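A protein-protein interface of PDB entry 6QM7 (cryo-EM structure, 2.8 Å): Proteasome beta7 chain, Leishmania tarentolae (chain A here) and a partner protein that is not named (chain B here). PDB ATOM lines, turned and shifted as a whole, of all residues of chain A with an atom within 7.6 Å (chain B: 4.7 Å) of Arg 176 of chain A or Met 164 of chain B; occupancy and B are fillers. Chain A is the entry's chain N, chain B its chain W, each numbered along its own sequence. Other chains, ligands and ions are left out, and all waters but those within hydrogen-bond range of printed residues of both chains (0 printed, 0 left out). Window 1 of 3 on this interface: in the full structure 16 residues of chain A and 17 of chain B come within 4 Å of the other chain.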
ATOM      1  N   TYR A 137     -15.134  27.340  -6.996  1.00  0.00           N
ATOM      2  CA  TYR A 137     -15.851  27.181  -8.280  1.00  0.00           C
ATOM      3  C   TYR A 137     -17.358  27.060  -8.030  1.00  0.00           C
ATOM      4  O   TYR A 137     -18.114  27.256  -8.972  1.00  0.00           O
ATOM      5  CB  TYR A 137     -15.236  26.026  -9.073  1.00  0.00           C
ATOM      6  CG  TYR A 137     -14.097  26.499  -9.929  1.00  0.00           C
ATOM      7  CD1 TYR A 137     -14.355  27.118 -11.146  1.00  0.00           C
ATOM      8  CD2 TYR A 137     -12.783  26.427  -9.497  1.00  0.00           C
ATOM      9  CE1 TYR A 137     -13.338  27.628 -11.935  1.00  0.00           C
ATOM     10  CE2 TYR A 137     -11.750  26.918 -10.282  1.00  0.00           C
ATOM     11  CZ  TYR A 137     -12.028  27.516 -11.506  1.00  0.00           C
ATOM     12  OH  TYR A 137     -11.040  28.012 -12.307  1.00  0.00           O
ATOM     13  N   TYR A 140     -18.969  30.190  -9.296  1.00  0.00           N
ATOM     14  CA  TYR A 140     -18.963  30.395 -10.762  1.00  0.00           C
ATOM     15  C   TYR A 140     -19.915  29.408 -11.419  1.00  0.00           C
ATOM     16  O   TYR A 140     -20.485  29.765 -12.453  1.00  0.00           O
ATOM     17  CB  TYR A 140     -17.532  30.280 -11.279  1.00  0.00           C
ATOM     18  CG  TYR A 140     -16.617  31.310 -10.668  1.00  0.00           C
ATOM     19  CD1 TYR A 140     -16.799  32.661 -10.926  1.00  0.00           C
ATOM     20  CD2 TYR A 140     -15.585  30.946  -9.818  1.00  0.00           C
ATOM     21  CE1 TYR A 140     -15.971  33.622 -10.367  1.00  0.00           C
ATOM     22  CE2 TYR A 140     -14.750  31.896  -9.247  1.00  0.00           C
ATOM     23  CZ  TYR A 140     -14.945  33.240  -9.518  1.00  0.00           C
ATOM     24  OH  TYR A 140     -14.127  34.184  -8.962  1.00  0.00           O
ATOM     25  N   ILE A 141     -20.083  28.228 -10.834  1.00  0.00           N
ATOM     26  CA  ILE A 141     -20.782  27.071 -11.454  1.00  0.00           C
ATOM     27  C   ILE A 141     -22.124  26.903 -10.763  1.00  0.00           C
ATOM     28  O   ILE A 141     -23.151  26.952 -11.428  1.00  0.00           O
ATOM     29  CB  ILE A 141     -19.925  25.805 -11.303  1.00  0.00           C
ATOM     30  CG1 ILE A 141     -18.686  25.870 -12.193  1.00  0.00           C
ATOM     31  CG2 ILE A 141     -20.733  24.538 -11.538  1.00  0.00           C
ATOM     32  CD1 ILE A 141     -17.606  24.886 -11.797  1.00  0.00           C
ATOM     33  N   LEU A 145     -27.116  28.256 -10.795  1.00  0.00           N
ATOM     34  CA  LEU A 145     -28.166  27.210 -10.744  1.00  0.00           C
ATOM     35  C   LEU A 145     -28.992  27.358  -9.480  1.00  0.00           C
ATOM     36  O   LEU A 145     -30.222  27.213  -9.580  1.00  0.00           O
ATOM     37  CB  LEU A 145     -27.533  25.821 -10.780  1.00  0.00           C
ATOM     38  CG  LEU A 145     -26.644  25.528 -11.985  1.00  0.00           C
ATOM     39  CD1 LEU A 145     -26.296  24.046 -12.022  1.00  0.00           C
ATOM     40  CD2 LEU A 145     -27.314  25.953 -13.282  1.00  0.00           C
ATOM     41  N   LEU A 170     -23.660  19.775  -7.311  1.00  0.00           N
ATOM     42  CA  LEU A 170     -22.509  18.902  -6.960  1.00  0.00           C
ATOM     43  C   LEU A 170     -22.110  18.115  -8.210  1.00  0.00           C
ATOM     44  O   LEU A 170     -20.907  18.050  -8.515  1.00  0.00           O
ATOM     45  CB  LEU A 170     -22.896  17.966  -5.809  1.00  0.00           C
ATOM     46  CG  LEU A 170     -23.228  18.666  -4.488  1.00  0.00           C
ATOM     47  CD1 LEU A 170     -23.577  17.665  -3.386  1.00  0.00           C
ATOM     48  CD2 LEU A 170     -22.091  19.586  -4.061  1.00  0.00           C
ATOM     49  N   ARG A 171     -23.093  17.564  -8.916  1.00  0.00           N
ATOM     50  CA  ARG A 171     -22.864  16.834 -10.186  1.00  0.00           C
ATOM     51  C   ARG A 171     -22.046  17.716 -11.120  1.00  0.00           C
ATOM     52  O   ARG A 171     -21.058  17.230 -11.651  1.00  0.00           O
ATOM     53  CB  ARG A 171     -24.177  16.443 -10.853  1.00  0.00           C
ATOM     54  CG  ARG A 171     -24.070  15.206 -11.725  1.00  0.00           C
ATOM     55  CD  ARG A 171     -25.352  14.946 -12.509  1.00  0.00           C
ATOM     56  NE  ARG A 171     -26.575  15.317 -11.802  1.00  0.00           N
ATOM     57  CZ  ARG A 171     -27.138  14.633 -10.808  1.00  0.00           C
ATOM     58  NH1 ARG A 171     -28.249  15.082 -10.250  1.00  0.00           N
ATOM     59  NH2 ARG A 171     -26.605  13.510 -10.367  1.00  0.00           N
ATOM     60  N   VAL A 172     -22.431  18.972 -11.280  1.00  0.00           N
ATOM     61  CA  VAL A 172     -21.772  19.880 -12.254  1.00  0.00           C
ATOM     62  C   VAL A 172     -20.381  20.227 -11.725  1.00  0.00           C
ATOM     63  O   VAL A 172     -19.446  20.306 -12.540  1.00  0.00           O
ATOM     64  CB  VAL A 172     -22.600  21.143 -12.524  1.00  0.00           C
ATOM     65  CG1 VAL A 172     -21.892  22.055 -13.517  1.00  0.00           C
ATOM     66  CG2 VAL A 172     -24.005  20.827 -13.012  1.00  0.00           C
ATOM     67  N   LEU A 173     -20.249  20.472 -10.424  1.00  0.00           N
ATOM     68  CA  LEU A 173     -18.935  20.760  -9.795  1.00  0.00           C
ATOM     69  C   LEU A 173     -18.006  19.588 -10.064  1.00  0.00           C
ATOM     70  O   LEU A 173     -16.836  19.820 -10.378  1.00  0.00           O
ATOM     71  CB  LEU A 173     -19.086  20.992  -8.291  1.00  0.00           C
ATOM     72  CG  LEU A 173     -19.576  22.386  -7.959  1.00  0.00           C
ATOM     73  CD1 LEU A 173     -20.051  22.461  -6.519  1.00  0.00           C
ATOM     74  CD2 LEU A 173     -18.496  23.422  -8.259  1.00  0.00           C
ATOM     75  N   PHE A 174     -18.531  18.377  -9.950  1.00  0.00           N
ATOM     76  CA  PHE A 174     -17.744  17.157 -10.197  1.00  0.00           C
ATOM     77  C   PHE A 174     -17.264  17.143 -11.643  1.00  0.00           C
ATOM     78  O   PHE A 174     -16.095  16.826 -11.855  1.00  0.00           O
ATOM     79  CB  PHE A 174     -18.534  15.895  -9.883  1.00  0.00           C
ATOM     80  CG  PHE A 174     -17.723  14.687 -10.238  1.00  0.00           C
ATOM     81  CD1 PHE A 174     -16.486  14.486  -9.640  1.00  0.00           C
ATOM     82  CD2 PHE A 174     -18.148  13.818 -11.231  1.00  0.00           C
ATOM     83  CE1 PHE A 174     -15.706  13.403  -9.993  1.00  0.00           C
ATOM     84  CE2 PHE A 174     -17.374  12.724 -11.575  1.00  0.00           C
ATOM     85  CZ  PHE A 174     -16.159  12.521 -10.950  1.00  0.00           C
ATOM     86  N   TYR A 175     -18.124  17.494 -12.596  1.00  0.00           N
ATOM     87  CA  TYR A 175     -17.792  17.506 -14.043  1.00  0.00           C
ATOM     88  C   TYR A 175     -16.752  18.577 -14.372  1.00  0.00           C
ATOM     89  O   TYR A 175     -15.917  18.315 -15.259  1.00  0.00           O
ATOM     90  CB  TYR A 175     -19.010  17.815 -14.896  1.00  0.00           C
ATOM     91  CG  TYR A 175     -20.123  16.800 -14.907  1.00  0.00           C
ATOM     92  CD1 TYR A 175     -19.902  15.435 -14.878  1.00  0.00           C
ATOM     93  CD2 TYR A 175     -21.431  17.233 -15.001  1.00  0.00           C
ATOM     94  CE1 TYR A 175     -20.958  14.532 -14.945  1.00  0.00           C
ATOM     95  CE2 TYR A 175     -22.493  16.351 -15.058  1.00  0.00           C
ATOM     96  CZ  TYR A 175     -22.260  14.992 -15.060  1.00  0.00           C
ATOM     97  OH  TYR A 175     -23.352  14.176 -15.123  1.00  0.00           O
ATOM     98  N   ARG A 176     -16.788  19.729 -13.693  1.00  0.00           N
ATOM     99  CA  ARG A 176     -16.161  20.984 -14.202  1.00  0.00           C
ATOM    100  C   ARG A 176     -15.083  21.551 -13.276  1.00  0.00           C
ATOM    101  O   ARG A 176     -14.160  22.166 -13.797  1.00  0.00           O
ATOM    102  CB  ARG A 176     -17.259  22.008 -14.499  1.00  0.00           C
ATOM    103  CG  ARG A 176     -18.187  21.574 -15.625  1.00  0.00           C
ATOM    104  CD  ARG A 176     -17.468  21.644 -16.948  1.00  0.00           C
ATOM    105  NE  ARG A 176     -18.084  20.865 -18.001  1.00  0.00           N
ATOM    106  CZ  ARG A 176     -17.721  20.930 -19.277  1.00  0.00           C
ATOM    107  NH1 ARG A 176     -16.745  21.736 -19.669  1.00  0.00           N
ATOM    108  NH2 ARG A 176     -18.335  20.177 -20.168  1.00  0.00           N
ATOM    109  N   GLU A 177     -15.212  21.415 -11.964  1.00  0.00           N
ATOM    110  CA  GLU A 177     -14.095  21.689 -11.029  1.00  0.00           C
ATOM    111  C   GLU A 177     -13.100  20.538 -11.216  1.00  0.00           C
ATOM    112  O   GLU A 177     -13.528  19.373 -11.152  1.00  0.00           O
ATOM    113  CB  GLU A 177     -14.643  21.847  -9.609  1.00  0.00           C
ATOM    114  CG  GLU A 177     -13.704  22.551  -8.634  1.00  0.00           C
ATOM    115  CD  GLU A 177     -14.164  22.647  -7.166  1.00  0.00           C
ATOM    116  OE1 GLU A 177     -14.787  21.670  -6.644  1.00  0.00           O
ATOM    117  OE2 GLU A 177     -13.880  23.697  -6.523  1.00  0.00           O
ATOM    118  N   CYS A 178     -11.844  20.842 -11.529  1.00  0.00           N
ATOM    119  CA  CYS A 178     -10.746  19.850 -11.657  1.00  0.00           C
ATOM    120  C   CYS A 178     -10.496  19.155 -10.317  1.00  0.00           C
ATOM    121  O   CYS A 178     -10.526  17.906 -10.267  1.00  0.00           O
ATOM    122  CB  CYS A 178      -9.442  20.512 -12.070  1.00  0.00           C
ATOM    123  SG  CYS A 178      -9.411  21.011 -13.806  1.00  0.00           S
ATOM    124  N   ARG A 179     -10.213  19.939  -9.278  1.00  0.00           N
ATOM    125  CA  ARG A 179      -9.809  19.435  -7.942  1.00  0.00           C
ATOM    126  C   ARG A 179     -11.070  19.118  -7.138  1.00  0.00           C
ATOM    127  O   ARG A 179     -11.354  19.799  -6.123  1.00  0.00           O
ATOM    128  CB  ARG A 179      -8.901  20.437  -7.228  1.00  0.00           C
ATOM    129  CG  ARG A 179      -7.464  20.404  -7.716  1.00  0.00           C
ATOM    130  CD  ARG A 179      -7.105  21.571  -8.596  1.00  0.00           C
ATOM    131  NE  ARG A 179      -6.187  22.492  -7.931  1.00  0.00           N
ATOM    132  CZ  ARG A 179      -5.008  22.889  -8.419  1.00  0.00           C
ATOM    133  NH1 ARG A 179      -4.278  23.752  -7.732  1.00  0.00           N
ATOM    134  NH2 ARG A 179      -4.553  22.450  -9.587  1.00  0.00           N
ATOM    135  N   ALA A 180     -11.788  18.102  -7.590  1.00  0.00           N
ATOM    136  CA  ALA A 180     -13.007  17.593  -6.948  1.00  0.00           C
ATOM    137  C   ALA A 180     -12.979  16.067  -6.969  1.00  0.00           C
ATOM    138  O   ALA A 180     -12.213  15.471  -7.751  1.00  0.00           O
ATOM    139  CB  ALA A 180     -14.220  18.137  -7.652  1.00  0.00           C
ATOM    140  N   TRP A 206     -21.939  10.233 -18.716  1.00  0.00           N
ATOM    141  CA  TRP A 206     -20.682  10.281 -19.505  1.00  0.00           C
ATOM    142  C   TRP A 206     -20.887   9.731 -20.922  1.00  0.00           C
ATOM    143  O   TRP A 206     -19.920   9.775 -21.702  1.00  0.00           O
ATOM    144  CB  TRP A 206     -19.626   9.465 -18.763  1.00  0.00           C
ATOM    145  CG  TRP A 206     -19.193  10.128 -17.504  1.00  0.00           C
ATOM    146  CD1 TRP A 206     -19.641   9.930 -16.228  1.00  0.00           C
ATOM    147  CD2 TRP A 206     -18.215  11.161 -17.433  1.00  0.00           C
ATOM    148  NE1 TRP A 206     -18.993  10.772 -15.364  1.00  0.00           N
ATOM    149  CE2 TRP A 206     -18.128  11.547 -16.082  1.00  0.00           C
ATOM    150  CE3 TRP A 206     -17.415  11.793 -18.395  1.00  0.00           C
ATOM    151  CZ2 TRP A 206     -17.253  12.546 -15.669  1.00  0.00           C
ATOM    152  CZ3 TRP A 206     -16.546  12.771 -17.985  1.00  0.00           C
ATOM    153  CH2 TRP A 206     -16.478  13.148 -16.642  1.00  0.00           C
ATOM    154  N   TYR A 211     -19.743  12.408 -27.160  1.00  0.00           N
ATOM    155  CA  TYR A 211     -18.503  12.128 -26.392  1.00  0.00           C
ATOM    156  C   TYR A 211     -17.839  10.867 -26.922  1.00  0.00           C
ATOM    157  O   TYR A 211     -16.768  10.514 -26.410  1.00  0.00           O
ATOM    158  CB  TYR A 211     -18.816  11.912 -24.908  1.00  0.00           C
ATOM    159  CG  TYR A 211     -19.091  13.147 -24.097  1.00  0.00           C
ATOM    160  CD1 TYR A 211     -19.281  13.048 -22.737  1.00  0.00           C
ATOM    161  CD2 TYR A 211     -19.120  14.406 -24.664  1.00  0.00           C
ATOM    162  CE1 TYR A 211     -19.520  14.169 -21.956  1.00  0.00           C
ATOM    163  CE2 TYR A 211     -19.362  15.533 -23.902  1.00  0.00           C
ATOM    164  CZ  TYR A 211     -19.564  15.423 -22.542  1.00  0.00           C
ATOM    165  OH  TYR A 211     -19.786  16.553 -21.795  1.00  0.00           O
ATOM    166  N   PHE B 153     -22.343  20.124 -26.614  1.00  0.00           N
ATOM    167  CA  PHE B 153     -22.689  21.444 -26.022  1.00  0.00           C
ATOM    168  C   PHE B 153     -21.413  22.145 -25.556  1.00  0.00           C
ATOM    169  O   PHE B 153     -20.571  21.519 -24.897  1.00  0.00           O
ATOM    170  CB  PHE B 153     -23.700  21.323 -24.878  1.00  0.00           C
ATOM    171  CG  PHE B 153     -23.270  20.413 -23.763  1.00  0.00           C
ATOM    172  CD1 PHE B 153     -22.689  20.922 -22.620  1.00  0.00           C
ATOM    173  CD2 PHE B 153     -23.407  19.040 -23.871  1.00  0.00           C
ATOM    174  CE1 PHE B 153     -22.277  20.081 -21.596  1.00  0.00           C
ATOM    175  CE2 PHE B 153     -23.001  18.196 -22.844  1.00  0.00           C
ATOM    176  CZ  PHE B 153     -22.426  18.720 -21.709  1.00  0.00           C
ATOM    177  N   VAL B 154     -21.296  23.424 -25.879  1.00  0.00           N
ATOM    178  CA  VAL B 154     -20.083  24.237 -25.617  1.00  0.00           C
ATOM    179  C   VAL B 154     -20.490  25.603 -25.102  1.00  0.00           C
ATOM    180  O   VAL B 154     -21.610  26.016 -25.370  1.00  0.00           O
ATOM    181  CB  VAL B 154     -19.258  24.409 -26.894  1.00  0.00           C
ATOM    182  CG1 VAL B 154     -18.807  23.069 -27.447  1.00  0.00           C
ATOM    183  CG2 VAL B 154     -20.005  25.225 -27.952  1.00  0.00           C
ATOM    184  N   THR B 155     -19.572  26.279 -24.431  1.00  0.00           N
ATOM    185  CA  THR B 155     -19.718  27.691 -24.012  1.00  0.00           C
ATOM    186  C   THR B 155     -18.365  28.370 -24.123  1.00  0.00           C
ATOM    187  O   THR B 155     -17.355  27.699 -23.953  1.00  0.00           O
ATOM    188  CB  THR B 155     -20.262  27.803 -22.586  1.00  0.00           C
ATOM    189  OG1 THR B 155     -19.258  27.354 -21.673  1.00  0.00           O
ATOM    190  CG2 THR B 155     -21.516  26.985 -22.377  1.00  0.00           C
ATOM    191  N   SER B 160     -19.008  31.814 -19.689  1.00  0.00           N
ATOM    192  CA  SER B 160     -18.921  30.411 -20.145  1.00  0.00           C
ATOM    193  C   SER B 160     -19.256  29.462 -19.001  1.00  0.00           C
ATOM    194  O   SER B 160     -19.986  28.497 -19.241  1.00  0.00           O
ATOM    195  CB  SER B 160     -17.565  30.081 -20.717  1.00  0.00           C
ATOM    196  OG  SER B 160     -16.530  30.264 -19.765  1.00  0.00           O
ATOM    197  N   ILE B 161     -18.703  29.710 -17.820  1.00  0.00           N
ATOM    198  CA  ILE B 161     -18.737  28.734 -16.698  1.00  0.00           C
ATOM    199  C   ILE B 161     -20.160  28.681 -16.133  1.00  0.00           C
ATOM    200  O   ILE B 161     -20.687  27.576 -15.946  1.00  0.00           O
ATOM    201  CB  ILE B 161     -17.673  29.096 -15.654  1.00  0.00           C
ATOM    202  CG1 ILE B 161     -16.272  28.967 -16.254  1.00  0.00           C
ATOM    203  CG2 ILE B 161     -17.853  28.247 -14.411  1.00  0.00           C
ATOM    204  CD1 ILE B 161     -15.136  29.195 -15.281  1.00  0.00           C
ATOM    205  N   ALA B 162     -20.765  29.835 -15.901  1.00  0.00           N
ATOM    206  CA  ALA B 162     -22.171  29.956 -15.462  1.00  0.00           C
ATOM    207  C   ALA B 162     -23.070  29.242 -16.467  1.00  0.00           C
ATOM    208  O   ALA B 162     -23.896  28.427 -16.025  1.00  0.00           O
ATOM    209  CB  ALA B 162     -22.552  31.409 -15.331  1.00  0.00           C
ATOM    210  N   ALA B 163     -22.904  29.539 -17.755  1.00  0.00           N
ATOM    211  CA  ALA B 163     -23.722  28.984 -18.852  1.00  0.00           C
ATOM    212  C   ALA B 163     -23.565  27.476 -18.877  1.00  0.00           C
ATOM    213  O   ALA B 163     -24.588  26.786 -18.929  1.00  0.00           O
ATOM    214  CB  ALA B 163     -23.307  29.563 -20.169  1.00  0.00           C
ATOM    215  N   MET B 164     -22.321  27.002 -18.823  1.00  0.00           N
ATOM    216  CA  MET B 164     -21.965  25.562 -18.903  1.00  0.00           C
ATOM    217  C   MET B 164     -22.631  24.820 -17.755  1.00  0.00           C
ATOM    218  O   MET B 164     -23.012  23.670 -17.949  1.00  0.00           O
ATOM    219  CB  MET B 164     -20.450  25.335 -18.826  1.00  0.00           C
ATOM    220  CG  MET B 164     -20.020  23.864 -18.896  1.00  0.00           C
ATOM    221  SD  MET B 164     -20.649  22.964 -20.346  1.00  0.00           S
ATOM    222  CE  MET B 164     -19.521  23.562 -21.600  1.00  0.00           C
ATOM    223  N   ALA B 165     -22.746  25.450 -16.594  1.00  0.00           N
ATOM    224  CA  ALA B 165     -23.405  24.826 -15.426  1.00  0.00           C
ATOM    225  C   ALA B 165     -24.840  24.469 -15.806  1.00  0.00           C
ATOM    226  O   ALA B 165     -25.256  23.341 -15.508  1.00  0.00           O
ATOM    227  CB  ALA B 165     -23.354  25.725 -14.224  1.00  0.00           C
ATOM    228  N   GLN B 166     -25.557  25.391 -16.447  1.00  0.00           N
ATOM    229  CA  GLN B 166     -26.955  25.152 -16.884  1.00  0.00           C
ATOM    230  C   GLN B 166     -26.964  24.020 -17.905  1.00  0.00           C
ATOM    231  O   GLN B 166     -27.856  23.175 -17.826  1.00  0.00           O
ATOM    232  CB  GLN B 166     -27.564  26.410 -17.500  1.00  0.00           C
ATOM    233  CG  GLN B 166     -28.986  26.221 -18.014  1.00  0.00           C
ATOM    234  CD  GLN B 166     -29.875  25.527 -17.014  1.00  0.00           C
ATOM    235  OE1 GLN B 166     -30.461  24.488 -17.305  1.00  0.00           O
ATOM    236  NE2 GLN B 166     -29.972  26.096 -15.824  1.00  0.00           N
ATOM    237  N   LEU B 167     -26.028  24.050 -18.849  1.00  0.00           N
ATOM    238  CA  LEU B 167     -25.928  23.054 -19.941  1.00  0.00           C
ATOM    239  C   LEU B 167     -25.678  21.658 -19.340  1.00  0.00           C
ATOM    240  O   LEU B 167     -26.462  20.757 -19.647  1.00  0.00           O
ATOM    241  CB  LEU B 167     -24.827  23.501 -20.906  1.00  0.00           C
ATOM    242  CG  LEU B 167     -25.255  24.112 -22.242  1.00  0.00           C
ATOM    243  CD1 LEU B 167     -26.644  24.706 -22.228  1.00  0.00           C
ATOM    244  CD2 LEU B 167     -24.251  25.160 -22.694  1.00  0.00           C
ATOM    245  N   GLU B 168     -24.665  21.488 -18.488  1.00  0.00           N
ATOM    246  CA  GLU B 168     -24.325  20.188 -17.839  1.00  0.00           C
ATOM    247  C   GLU B 168     -25.522  19.660 -17.037  1.00  0.00           C
ATOM    248  O   GLU B 168     -25.696  18.437 -16.955  1.00  0.00           O
ATOM    249  CB  GLU B 168     -23.132  20.331 -16.891  1.00  0.00           C
ATOM    250  CG  GLU B 168     -21.776  20.339 -17.578  1.00  0.00           C
ATOM    251  CD  GLU B 168     -21.358  19.014 -18.202  1.00  0.00           C
ATOM    252  OE1 GLU B 168     -22.148  18.015 -18.132  1.00  0.00           O
ATOM    253  OE2 GLU B 168     -20.239  18.978 -18.782  1.00  0.00           O
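O of Tyr 140 of chain A sits close to N of Ala 162 of chain B (3.5 Å).
The guanidinium group (NH2) of Arg 176 of chain A sits at hydrogen-bond distance from the side-chain sulfur (SD) of Met 164 of chain B (3.6 Å).
NH2 of Arg 176 of chain A is in salt-bridge range of OE2 of Glu 168 of chain B, 2.6 Å away.
Ile 161 of chain B touches Tyr 140 of chain A.
Ile 141 of chain A touches Ile 161 of chain B.
O of Ile 141 of chain A touches CB of Ala 165 of chain B (3.1 Å).
Leu 145 of chain A touches Ala 165 of chain B.
N of Gln 166 of chain B touches CD2 of Leu 145 of chain A (3.7 Å).
Ala 165 of chain B touches Val 172 of chain A (CA to CG1, 3.7 Å).
CG1 of Val 172 of chain A touches CB of Glu 168 of chain B, 3.99 Å away.
Glu 168 of chain B touches Tyr 175 of chain A.
Tyr 211 of chain A touches Phe 153 of chain B (OH to CZ, 3.4 Å).
Tyr 211 of chain A touches Glu 168 of chain B (OH to OE2, 3.9 Å).
Arg 176 of chain A touches two residues of chain B.
Of the printed residues of chain A, Met 164 of chain B touches Arg 176.
Ala 163 of chain B touches none of the printed residues of chain A.
Printed residues of chain B within 4 Å of Tyr 211 of chain A: Phe 153 (3.4 Å) and Glu 168 (3.9 Å).
Of the printed residues of chain B, Tyr 175 of chain A touches Glu 168.
Printed residues of chain A within 4 Å of Ala 165 of chain B: Ile 141 (3.1 Å), Leu 145 (3.7 Å) and Val 172 (3.7 Å).
The nearest residue of chain B that does not touch Arg 176 of chain A is Phe 153 of chain B (4.2 Å).
The nearest residue of chain A that does not touch Met 164 of chain B is Val 172 of chain A (4.8 Å).
The nearest printed residue of chain A that does not touch Ile 161 of chain B is Tyr 137 of chain A (4.1 Å).
Printed residues of chain A that touch a printed residue of chain B: Tyr 140, Ile 141, Leu 145, Val 172, Tyr 175, Arg 176 and Tyr 211.
Hydrophobic or aromatic side chains of chain A within 4 Å of the printed part of chain B: Tyr 140, Ile 141, Leu 145, Val 172, Tyr 175 and Tyr 211.
Of the 12 printed residues of chain B, 7 touch a printed residue of chain A.
Hydrophobic or aromatic side chains of chain B that line the printed part of chain A: Phe 153, Ile 161, Ala 162, Met 164 and Ala 165.
Among the printed residues, 13 pairs touch across the chains.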
